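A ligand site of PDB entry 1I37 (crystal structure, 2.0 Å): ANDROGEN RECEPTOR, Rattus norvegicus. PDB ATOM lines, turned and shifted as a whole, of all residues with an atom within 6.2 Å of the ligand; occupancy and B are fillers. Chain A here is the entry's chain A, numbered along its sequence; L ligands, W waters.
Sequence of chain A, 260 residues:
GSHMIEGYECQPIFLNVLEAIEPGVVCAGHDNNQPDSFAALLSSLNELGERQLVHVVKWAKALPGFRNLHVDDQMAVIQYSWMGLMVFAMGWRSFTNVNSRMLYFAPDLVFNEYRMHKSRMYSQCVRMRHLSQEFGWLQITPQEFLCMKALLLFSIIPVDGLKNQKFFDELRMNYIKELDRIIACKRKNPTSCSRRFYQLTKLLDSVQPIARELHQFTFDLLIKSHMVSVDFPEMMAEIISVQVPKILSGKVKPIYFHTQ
An oxygen (O2) of the ligand is in hydrogen-bond range of the side-chain amide nitrogen (ND2) of Asn 46 (2.8 Å). OE1 of Gln 52 sits close to O1 of the ligand. An oxygen (O2) of the ligand sits at hydrogen-bond distance from the side-chain hydroxyl (OG1) of Thr 218 (2.7 Å). An oxygen (O1) of the ligand lies within hydrogen-bond range of the guanidinium group (NH2) of Arg 93 (2.9 Å).
NH2 of Arg 93 lies within hydrogen-bond range of O of Phe 105, at 3.0 Å. OD1 of Asn 46 lies close to O of Leu 42 (3.1 Å). The guanidinium group (NH2) of Arg 93 lies within hydrogen-bond range of the side-chain amide oxygen (OE1) of Gln 52, at 3.2 Å. The guanidinium group (NE) of Arg 93 sits at hydrogen-bond distance from the backbone carbonyl oxygen (O) of Tyr 104 (3.2 Å).
Residues that only touch the ligand: Leu 42, Leu 45, Leu 48, Gly 49, Trp 82, Met 83, Met 86, Met 90, Phe 105, Met 121, Met 128, Leu 214, Phe 217, Leu 221, Phe 232 and Met 236. Hydrophobic or aromatic side chains that line the ligand: Leu 42, Leu 48, Trp 82, Met 83, Met 86, Met 90, Phe 105, Met 121, Met 128, Leu 214, Phe 217, Leu 221, Phe 232 and Met 236. 20 residues have an atom within 4 Å of the ligand: Leu 42, Leu 45, Asn 46, Leu 48, Gly 49, Gln 52, Trp 82, Met 83, Met 86, Met 90, Arg 93, Phe 105, Met 121, Met 128, Leu 214, Phe 217, Thr 218, Leu 221, Phe 232 and Met 236. The nearest printed residue that does not touch the ligand is Val 87 (4.2 Å).
Water W1 lies within hydrogen-bond range of the side-chain amide nitrogen (NE2) of Gln 52 (2.6 Å), the guanidinium group (NH1) of Arg 93 (2.7 Å), the backbone carbonyl oxygen (O) of Met 86 (2.7 Å) and an oxygen (O1) of the ligand (3.5 Å).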
ATOM      1  N   LEU A  42      26.166  22.907 -16.225  1.00  0.00           N
ATOM      2  CA  LEU A  42      25.940  21.915 -17.242  1.00  0.00           C
ATOM      3  C   LEU A  42      26.428  20.552 -16.844  1.00  0.00           C
ATOM      4  O   LEU A  42      25.855  19.552 -17.228  1.00  0.00           O
ATOM      5  CB  LEU A  42      26.426  22.397 -18.605  1.00  0.00           C
ATOM      6  CG  LEU A  42      25.141  23.077 -19.096  1.00  0.00           C
ATOM      7  CD1 LEU A  42      25.313  24.527 -19.276  1.00  0.00           C
ATOM      8  CD2 LEU A  42      24.602  22.416 -20.310  1.00  0.00           C
ATOM      9  N   LEU A  45      23.486  19.360 -14.836  1.00  0.00           N
ATOM     10  CA  LEU A  45      22.347  18.936 -15.632  1.00  0.00           C
ATOM     11  C   LEU A  45      22.629  17.583 -16.257  1.00  0.00           C
ATOM     12  O   LEU A  45      21.716  16.759 -16.351  1.00  0.00           O
ATOM     13  CB  LEU A  45      22.018  19.960 -16.714  1.00  0.00           C
ATOM     14  CG  LEU A  45      21.268  21.204 -16.297  1.00  0.00           C
ATOM     15  CD1 LEU A  45      21.228  22.165 -17.431  1.00  0.00           C
ATOM     16  CD2 LEU A  45      19.855  20.823 -15.843  1.00  0.00           C
ATOM     17  N   ASN A  46      23.879  17.351 -16.659  1.00  0.00           N
ATOM     18  CA  ASN A  46      24.306  16.084 -17.277  1.00  0.00           C
ATOM     19  C   ASN A  46      24.239  14.917 -16.286  1.00  0.00           C
ATOM     20  O   ASN A  46      23.777  13.838 -16.632  1.00  0.00           O
ATOM     21  CB  ASN A  46      25.725  16.177 -17.850  1.00  0.00           C
ATOM     22  CG  ASN A  46      25.805  17.035 -19.095  1.00  0.00           C
ATOM     23  OD1 ASN A  46      26.839  17.600 -19.373  1.00  0.00           O
ATOM     24  ND2 ASN A  46      24.729  17.118 -19.838  1.00  0.00           N
ATOM     25  N   GLU A  47      24.715  15.137 -15.074  1.00  0.00           N
ATOM     26  CA  GLU A  47      24.700  14.128 -14.006  1.00  0.00           C
ATOM     27  C   GLU A  47      23.248  13.794 -13.684  1.00  0.00           C
ATOM     28  O   GLU A  47      22.865  12.638 -13.471  1.00  0.00           O
ATOM     29  CB  GLU A  47      25.387  14.692 -12.747  1.00  0.00           C
ATOM     30  CG  GLU A  47      25.404  13.780 -11.546  1.00  0.00           C
ATOM     31  CD  GLU A  47      26.028  12.406 -11.849  1.00  0.00           C
ATOM     32  OE1 GLU A  47      25.515  11.395 -11.333  1.00  0.00           O
ATOM     33  OE2 GLU A  47      27.023  12.330 -12.605  1.00  0.00           O
ATOM     34  N   LEU A  48      22.444  14.844 -13.627  1.00  0.00           N
ATOM     35  CA  LEU A  48      21.023  14.700 -13.371  1.00  0.00           C
ATOM     36  C   LEU A  48      20.452  13.863 -14.487  1.00  0.00           C
ATOM     37  O   LEU A  48      19.578  13.017 -14.235  1.00  0.00           O
ATOM     38  CB  LEU A  48      20.346  16.062 -13.377  1.00  0.00           C
ATOM     39  CG  LEU A  48      18.842  16.010 -13.311  1.00  0.00           C
ATOM     40  CD1 LEU A  48      18.453  15.290 -12.056  1.00  0.00           C
ATOM     41  CD2 LEU A  48      18.314  17.396 -13.264  1.00  0.00           C
ATOM     42  N   GLY A  49      20.924  14.111 -15.700  1.00  0.00           N
ATOM     43  CA  GLY A  49      20.445  13.358 -16.835  1.00  0.00           C
ATOM     44  C   GLY A  49      20.786  11.891 -16.682  1.00  0.00           C
ATOM     45  O   GLY A  49      20.004  11.025 -17.008  1.00  0.00           O
ATOM     46  N   GLN A  52      18.404  10.530 -13.762  1.00  0.00           N
ATOM     47  CA  GLN A  52      17.048  10.400 -14.240  1.00  0.00           C
ATOM     48  C   GLN A  52      16.867   9.293 -15.261  1.00  0.00           C
ATOM     49  O   GLN A  52      15.807   8.661 -15.283  1.00  0.00           O
ATOM     50  CB  GLN A  52      16.508  11.716 -14.777  1.00  0.00           C
ATOM     51  CG  GLN A  52      16.130  12.641 -13.663  1.00  0.00           C
ATOM     52  CD  GLN A  52      15.317  13.813 -14.118  1.00  0.00           C
ATOM     53  OE1 GLN A  52      15.414  14.921 -13.551  1.00  0.00           O
ATOM     54  NE2 GLN A  52      14.463  13.584 -15.087  1.00  0.00           N
ATOM     55  N   TRP A  82      14.189   9.753 -24.226  1.00  0.00           N
ATOM     56  CA  TRP A  82      14.493  10.345 -22.930  1.00  0.00           C
ATOM     57  C   TRP A  82      14.419  11.873 -22.853  1.00  0.00           C
ATOM     58  O   TRP A  82      13.833  12.406 -21.913  1.00  0.00           O
ATOM     59  CB  TRP A  82      15.823   9.812 -22.360  1.00  0.00           C
ATOM     60  CG  TRP A  82      17.023  10.134 -23.178  1.00  0.00           C
ATOM     61  CD1 TRP A  82      17.501   9.414 -24.215  1.00  0.00           C
ATOM     62  CD2 TRP A  82      17.904  11.258 -23.022  1.00  0.00           C
ATOM     63  NE1 TRP A  82      18.602  10.025 -24.747  1.00  0.00           N
ATOM     64  CE2 TRP A  82      18.885  11.157 -24.036  1.00  0.00           C
ATOM     65  CE3 TRP A  82      17.967  12.348 -22.132  1.00  0.00           C
ATOM     66  CZ2 TRP A  82      19.910  12.094 -24.186  1.00  0.00           C
ATOM     67  CZ3 TRP A  82      18.992  13.286 -22.282  1.00  0.00           C
ATOM     68  CH2 TRP A  82      19.939  13.161 -23.301  1.00  0.00           C
ATOM     69  N   MET A  83      14.922  12.611 -23.852  1.00  0.00           N
ATOM     70  CA  MET A  83      14.883  14.068 -23.784  1.00  0.00           C
ATOM     71  C   MET A  83      13.509  14.650 -23.625  1.00  0.00           C
ATOM     72  O   MET A  83      13.297  15.500 -22.769  1.00  0.00           O
ATOM     73  CB  MET A  83      15.546  14.720 -24.988  1.00  0.00           C
ATOM     74  CG  MET A  83      15.657  16.241 -24.884  1.00  0.00           C
ATOM     75  SD  MET A  83      16.944  16.707 -23.778  1.00  0.00           S
ATOM     76  CE  MET A  83      18.346  16.511 -24.846  1.00  0.00           C
ATOM     77  N   MET A  86      11.974  13.613 -20.110  1.00  0.00           N
ATOM     78  CA  MET A  86      12.552  14.359 -18.978  1.00  0.00           C
ATOM     79  C   MET A  86      12.144  15.827 -18.976  1.00  0.00           C
ATOM     80  O   MET A  86      11.952  16.419 -17.918  1.00  0.00           O
ATOM     81  CB  MET A  86      14.071  14.271 -18.965  1.00  0.00           C
ATOM     82  CG  MET A  86      14.600  12.849 -18.842  1.00  0.00           C
ATOM     83  SD  MET A  86      16.325  12.849 -18.626  1.00  0.00           S
ATOM     84  CE  MET A  86      16.723  11.191 -18.713  1.00  0.00           C
ATOM     85  N   VAL A  87      12.010  16.394 -20.178  1.00  0.00           N
ATOM     86  CA  VAL A  87      11.621  17.775 -20.366  1.00  0.00           C
ATOM     87  C   VAL A  87      10.174  17.962 -19.950  1.00  0.00           C
ATOM     88  O   VAL A  87       9.836  18.926 -19.295  1.00  0.00           O
ATOM     89  CB  VAL A  87      11.746  18.172 -21.845  1.00  0.00           C
ATOM     90  CG1 VAL A  87      10.983  19.433 -22.112  1.00  0.00           C
ATOM     91  CG2 VAL A  87      13.183  18.367 -22.215  1.00  0.00           C
ATOM     92  N   MET A  90       9.854  17.569 -16.204  1.00  0.00           N
ATOM     93  CA  MET A  90      10.499  18.721 -15.587  1.00  0.00           C
ATOM     94  C   MET A  90       9.559  19.908 -15.635  1.00  0.00           C
ATOM     95  O   MET A  90       9.530  20.720 -14.709  1.00  0.00           O
ATOM     96  CB  MET A  90      11.800  19.028 -16.326  1.00  0.00           C
ATOM     97  CG  MET A  90      12.671  20.127 -15.763  1.00  0.00           C
ATOM     98  SD  MET A  90      12.084  21.798 -15.988  1.00  0.00           S
ATOM     99  CE  MET A  90      12.480  22.056 -17.671  1.00  0.00           C
ATOM    100  N   ARG A  93       6.996  19.368 -12.747  1.00  0.00           N
ATOM    101  CA  ARG A  93       7.562  19.736 -11.445  1.00  0.00           C
ATOM    102  C   ARG A  93       7.621  21.236 -11.253  1.00  0.00           C
ATOM    103  O   ARG A  93       7.429  21.739 -10.144  1.00  0.00           O
ATOM    104  CB  ARG A  93       8.973  19.211 -11.329  1.00  0.00           C
ATOM    105  CG  ARG A  93       9.079  17.733 -11.438  1.00  0.00           C
ATOM    106  CD  ARG A  93      10.463  17.264 -11.017  1.00  0.00           C
ATOM    107  NE  ARG A  93      11.528  17.606 -11.955  1.00  0.00           N
ATOM    108  CZ  ARG A  93      11.925  16.816 -12.946  1.00  0.00           C
ATOM    109  NH1 ARG A  93      11.325  15.658 -13.155  1.00  0.00           N
ATOM    110  NH2 ARG A  93      13.019  17.100 -13.626  1.00  0.00           N
ATOM    111  N   TYR A 104      12.183  23.880 -12.427  1.00  0.00           N
ATOM    112  CA  TYR A 104      12.513  22.943 -11.358  1.00  0.00           C
ATOM    113  C   TYR A 104      13.122  21.665 -11.890  1.00  0.00           C
ATOM    114  O   TYR A 104      12.441  20.650 -11.973  1.00  0.00           O
ATOM    115  CB  TYR A 104      11.237  22.602 -10.602  1.00  0.00           C
ATOM    116  CG  TYR A 104      11.476  22.094  -9.214  1.00  0.00           C
ATOM    117  CD1 TYR A 104      11.572  22.985  -8.156  1.00  0.00           C
ATOM    118  CD2 TYR A 104      11.531  20.725  -8.937  1.00  0.00           C
ATOM    119  CE1 TYR A 104      11.725  22.542  -6.851  1.00  0.00           C
ATOM    120  CE2 TYR A 104      11.681  20.261  -7.620  1.00  0.00           C
ATOM    121  CZ  TYR A 104      11.766  21.187  -6.586  1.00  0.00           C
ATOM    122  OH  TYR A 104      11.831  20.778  -5.269  1.00  0.00           O
ATOM    123  N   PHE A 105      14.418  21.707 -12.178  1.00  0.00           N
ATOM    124  CA  PHE A 105      15.121  20.563 -12.726  1.00  0.00           C
ATOM    125  C   PHE A 105      15.287  19.528 -11.657  1.00  0.00           C
ATOM    126  O   PHE A 105      15.210  18.319 -11.921  1.00  0.00           O
ATOM    127  CB  PHE A 105      16.506  20.974 -13.190  1.00  0.00           C
ATOM    128  CG  PHE A 105      16.496  21.727 -14.476  1.00  0.00           C
ATOM    129  CD1 PHE A 105      16.845  23.049 -14.513  1.00  0.00           C
ATOM    130  CD2 PHE A 105      16.162  21.083 -15.652  1.00  0.00           C
ATOM    131  CE1 PHE A 105      16.860  23.730 -15.713  1.00  0.00           C
ATOM    132  CE2 PHE A 105      16.170  21.752 -16.851  1.00  0.00           C
ATOM    133  CZ  PHE A 105      16.522  23.082 -16.882  1.00  0.00           C
ATOM    134  N   ALA A 106      15.561  19.996 -10.458  1.00  0.00           N
ATOM    135  CA  ALA A 106      15.772  19.120  -9.328  1.00  0.00           C
ATOM    136  C   ALA A 106      15.583  20.020  -8.146  1.00  0.00           C
ATOM    137  O   ALA A 106      15.525  21.234  -8.298  1.00  0.00           O
ATOM    138  CB  ALA A 106      17.174  18.567  -9.346  1.00  0.00           C
ATOM    139  N   MET A 121      21.792  28.671 -22.446  1.00  0.00           N
ATOM    140  CA  MET A 121      20.591  27.942 -22.830  1.00  0.00           C
ATOM    141  C   MET A 121      19.317  28.758 -22.740  1.00  0.00           C
ATOM    142  O   MET A 121      18.217  28.194 -22.782  1.00  0.00           O
ATOM    143  CB  MET A 121      20.431  26.696 -21.968  1.00  0.00           C
ATOM    144  CG  MET A 121      20.936  25.429 -22.571  1.00  0.00           C
ATOM    145  SD  MET A 121      20.740  24.077 -21.423  1.00  0.00           S
ATOM    146  CE  MET A 121      19.094  23.671 -21.739  1.00  0.00           C
ATOM    147  N   MET A 128      10.832  25.712 -22.436  1.00  0.00           N
ATOM    148  CA  MET A 128      10.450  24.721 -21.430  1.00  0.00           C
ATOM    149  C   MET A 128       9.608  25.347 -20.354  1.00  0.00           C
ATOM    150  O   MET A 128       8.745  24.689 -19.766  1.00  0.00           O
ATOM    151  CB  MET A 128      11.678  24.097 -20.811  1.00  0.00           C
ATOM    152  CG  MET A 128      12.391  23.171 -21.733  1.00  0.00           C
ATOM    153  SD  MET A 128      14.043  22.845 -21.160  1.00  0.00           S
ATOM    154  CE  MET A 128      13.955  21.308 -20.674  1.00  0.00           C
ATOM    155  N   LEU A 214      17.374  20.839 -27.846  1.00  0.00           N
ATOM    156  CA  LEU A 214      18.262  20.362 -26.791  1.00  0.00           C
ATOM    157  C   LEU A 214      19.177  19.274 -27.288  1.00  0.00           C
ATOM    158  O   LEU A 214      20.307  19.157 -26.823  1.00  0.00           O
ATOM    159  CB  LEU A 214      17.460  19.897 -25.565  1.00  0.00           C
ATOM    160  CG  LEU A 214      16.647  21.009 -24.903  1.00  0.00           C
ATOM    161  CD1 LEU A 214      15.543  20.472 -24.031  1.00  0.00           C
ATOM    162  CD2 LEU A 214      17.578  21.935 -24.131  1.00  0.00           C
ATOM    163  N   PHE A 217      21.847  20.973 -29.014  1.00  0.00           N
ATOM    164  CA  PHE A 217      22.649  21.641 -27.988  1.00  0.00           C
ATOM    165  C   PHE A 217      23.536  20.657 -27.278  1.00  0.00           C
ATOM    166  O   PHE A 217      24.758  20.825 -27.246  1.00  0.00           O
ATOM    167  CB  PHE A 217      21.760  22.344 -26.942  1.00  0.00           C
ATOM    168  CG  PHE A 217      22.550  23.164 -25.925  1.00  0.00           C
ATOM    169  CD1 PHE A 217      23.232  22.543 -24.892  1.00  0.00           C
ATOM    170  CD2 PHE A 217      22.602  24.548 -26.027  1.00  0.00           C
ATOM    171  CE1 PHE A 217      23.961  23.300 -23.953  1.00  0.00           C
ATOM    172  CE2 PHE A 217      23.331  25.305 -25.088  1.00  0.00           C
ATOM    173  CZ  PHE A 217      24.013  24.684 -24.055  1.00  0.00           C
ATOM    174  N   THR A 218      22.935  19.590 -26.750  1.00  0.00           N
ATOM    175  CA  THR A 218      23.717  18.612 -26.015  1.00  0.00           C
ATOM    176  C   THR A 218      24.788  18.005 -26.892  1.00  0.00           C
ATOM    177  O   THR A 218      25.905  17.773 -26.422  1.00  0.00           O
ATOM    178  CB  THR A 218      22.851  17.515 -25.337  1.00  0.00           C
ATOM    179  OG1 THR A 218      23.579  16.970 -24.237  1.00  0.00           O
ATOM    180  CG2 THR A 218      22.496  16.384 -26.296  1.00  0.00           C
ATOM    181  N   PHE A 219      24.441  17.705 -28.146  1.00  0.00           N
ATOM    182  CA  PHE A 219      25.420  17.137 -29.084  1.00  0.00           C
ATOM    183  C   PHE A 219      26.644  18.061 -29.292  1.00  0.00           C
ATOM    184  O   PHE A 219      27.785  17.623 -29.150  1.00  0.00           O
ATOM    185  CB  PHE A 219      24.777  16.868 -30.432  1.00  0.00           C
ATOM    186  CG  PHE A 219      25.764  16.408 -31.468  1.00  0.00           C
ATOM    187  CD1 PHE A 219      26.186  15.089 -31.504  1.00  0.00           C
ATOM    188  CD2 PHE A 219      26.303  17.320 -32.389  1.00  0.00           C
ATOM    189  CE1 PHE A 219      27.136  14.669 -32.437  1.00  0.00           C
ATOM    190  CE2 PHE A 219      27.254  16.924 -33.321  1.00  0.00           C
ATOM    191  CZ  PHE A 219      27.676  15.605 -33.357  1.00  0.00           C
ATOM    192  N   LEU A 221      27.594  20.383 -27.394  1.00  0.00           N
ATOM    193  CA  LEU A 221      28.291  20.475 -26.130  1.00  0.00           C
ATOM    194  C   LEU A 221      29.239  19.317 -25.950  1.00  0.00           C
ATOM    195  O   LEU A 221      30.372  19.514 -25.546  1.00  0.00           O
ATOM    196  CB  LEU A 221      27.292  20.515 -24.971  1.00  0.00           C
ATOM    197  CG  LEU A 221      27.909  20.925 -23.645  1.00  0.00           C
ATOM    198  CD1 LEU A 221      28.815  22.134 -23.828  1.00  0.00           C
ATOM    199  CD2 LEU A 221      26.786  21.214 -22.697  1.00  0.00           C
ATOM    200  N   VAL A 230      33.038  20.929 -19.379  1.00  0.00           N
ATOM    201  CA  VAL A 230      31.777  20.306 -18.984  1.00  0.00           C
ATOM    202  C   VAL A 230      31.964  18.842 -19.219  1.00  0.00           C
ATOM    203  O   VAL A 230      32.518  18.497 -20.259  1.00  0.00           O
ATOM    204  CB  VAL A 230      30.603  20.743 -19.918  1.00  0.00           C
ATOM    205  CG1 VAL A 230      29.318  20.013 -19.557  1.00  0.00           C
ATOM    206  CG2 VAL A 230      30.384  22.213 -19.833  1.00  0.00           C
ATOM    207  N   PHE A 232      30.384  14.847 -19.466  1.00  0.00           N
ATOM    208  CA  PHE A 232      29.225  13.995 -19.598  1.00  0.00           C
ATOM    209  C   PHE A 232      29.481  12.643 -18.998  1.00  0.00           C
ATOM    210  O   PHE A 232      30.492  12.003 -19.310  1.00  0.00           O
ATOM    211  CB  PHE A 232      28.896  13.829 -21.094  1.00  0.00           C
ATOM    212  CG  PHE A 232      28.426  15.089 -21.764  1.00  0.00           C
ATOM    213  CD1 PHE A 232      29.281  16.160 -21.926  1.00  0.00           C
ATOM    214  CD2 PHE A 232      27.133  15.210 -22.209  1.00  0.00           C
ATOM    215  CE1 PHE A 232      28.850  17.345 -22.531  1.00  0.00           C
ATOM    216  CE2 PHE A 232      26.695  16.359 -22.813  1.00  0.00           C
ATOM    217  CZ  PHE A 232      27.568  17.445 -22.970  1.00  0.00           C
ATOM    218  N   MET A 236      25.376   9.172 -20.745  1.00  0.00           N
ATOM    219  CA  MET A 236      25.062  10.403 -21.467  1.00  0.00           C
ATOM    220  C   MET A 236      25.934  10.520 -22.726  1.00  0.00           C
ATOM    221  O   MET A 236      25.423  10.621 -23.815  1.00  0.00           O
ATOM    222  CB  MET A 236      25.253  11.625 -20.589  1.00  0.00           C
ATOM    223  CG  MET A 236      24.179  11.809 -19.538  1.00  0.00           C
ATOM    224  SD  MET A 236      22.533  11.938 -20.230  1.00  0.00           S
ATOM    225  CE  MET A 236      22.336  13.650 -20.312  1.00  0.00           C
ATOM    226  N   ILE A 240      24.529  10.146 -26.379  1.00  0.00           N
ATOM    227  CA  ILE A 240      24.565  11.373 -27.139  1.00  0.00           C
ATOM    228  C   ILE A 240      25.416  11.262 -28.412  1.00  0.00           C
ATOM    229  O   ILE A 240      25.122  11.899 -29.405  1.00  0.00           O
ATOM    230  CB  ILE A 240      24.983  12.555 -26.245  1.00  0.00           C
ATOM    231  CG1 ILE A 240      23.960  12.757 -25.120  1.00  0.00           C
ATOM    232  CG2 ILE A 240      25.065  13.843 -27.074  1.00  0.00           C
ATOM    233  CD1 ILE A 240      24.341  13.814 -24.090  1.00  0.00           C
HETATM  234  C1  LIG L   1      18.029  16.366 -17.346  1.00  0.00           C
HETATM  235  C2  LIG L   1      16.735  16.128 -16.528  1.00  0.00           C
HETATM  236  C3  LIG L   1      15.842  17.353 -16.544  1.00  0.00           C
HETATM  237  O1  LIG L   1      15.077  17.558 -15.600  1.00  0.00           O
HETATM  238  C4  LIG L   1      15.877  18.266 -17.667  1.00  0.00           C
HETATM  239  C5  LIG L   1      16.666  18.097 -18.690  1.00  0.00           C
HETATM  240  C6  LIG L   1      16.598  19.113 -19.833  1.00  0.00           C
HETATM  241  C7  LIG L   1      17.985  19.706 -20.194  1.00  0.00           C
HETATM  242  C8  LIG L   1      19.023  18.590 -20.483  1.00  0.00           C
HETATM  243  C9  LIG L   1      19.154  17.711 -19.207  1.00  0.00           C
HETATM  244  C10 LIG L   1      17.809  16.989 -18.759  1.00  0.00           C
HETATM  245  C11 LIG L   1      20.330  16.701 -19.355  1.00  0.00           C
HETATM  246  C12 LIG L   1      21.669  17.373 -19.783  1.00  0.00           C
HETATM  247  C13 LIG L   1      21.505  18.197 -21.093  1.00  0.00           C
HETATM  248  C14 LIG L   1      20.362  19.239 -20.811  1.00  0.00           C
HETATM  249  C15 LIG L   1      20.424  20.172 -22.060  1.00  0.00           C
HETATM  250  C16 LIG L   1      21.976  20.272 -22.338  1.00  0.00           C
HETATM  251  C17 LIG L   1      22.654  19.212 -21.426  1.00  0.00           C
HETATM  252  O2  LIG L   1      23.875  18.563 -22.087  1.00  0.00           O
HETATM  253  C18 LIG L   1      21.203  17.256 -22.320  1.00  0.00           C
HETATM  254  C19 LIG L   1      17.288  15.891 -19.771  1.00  0.00           C
HETATM  255  O   HOH W   1      12.499  15.258 -15.540  1.00  0.00           O
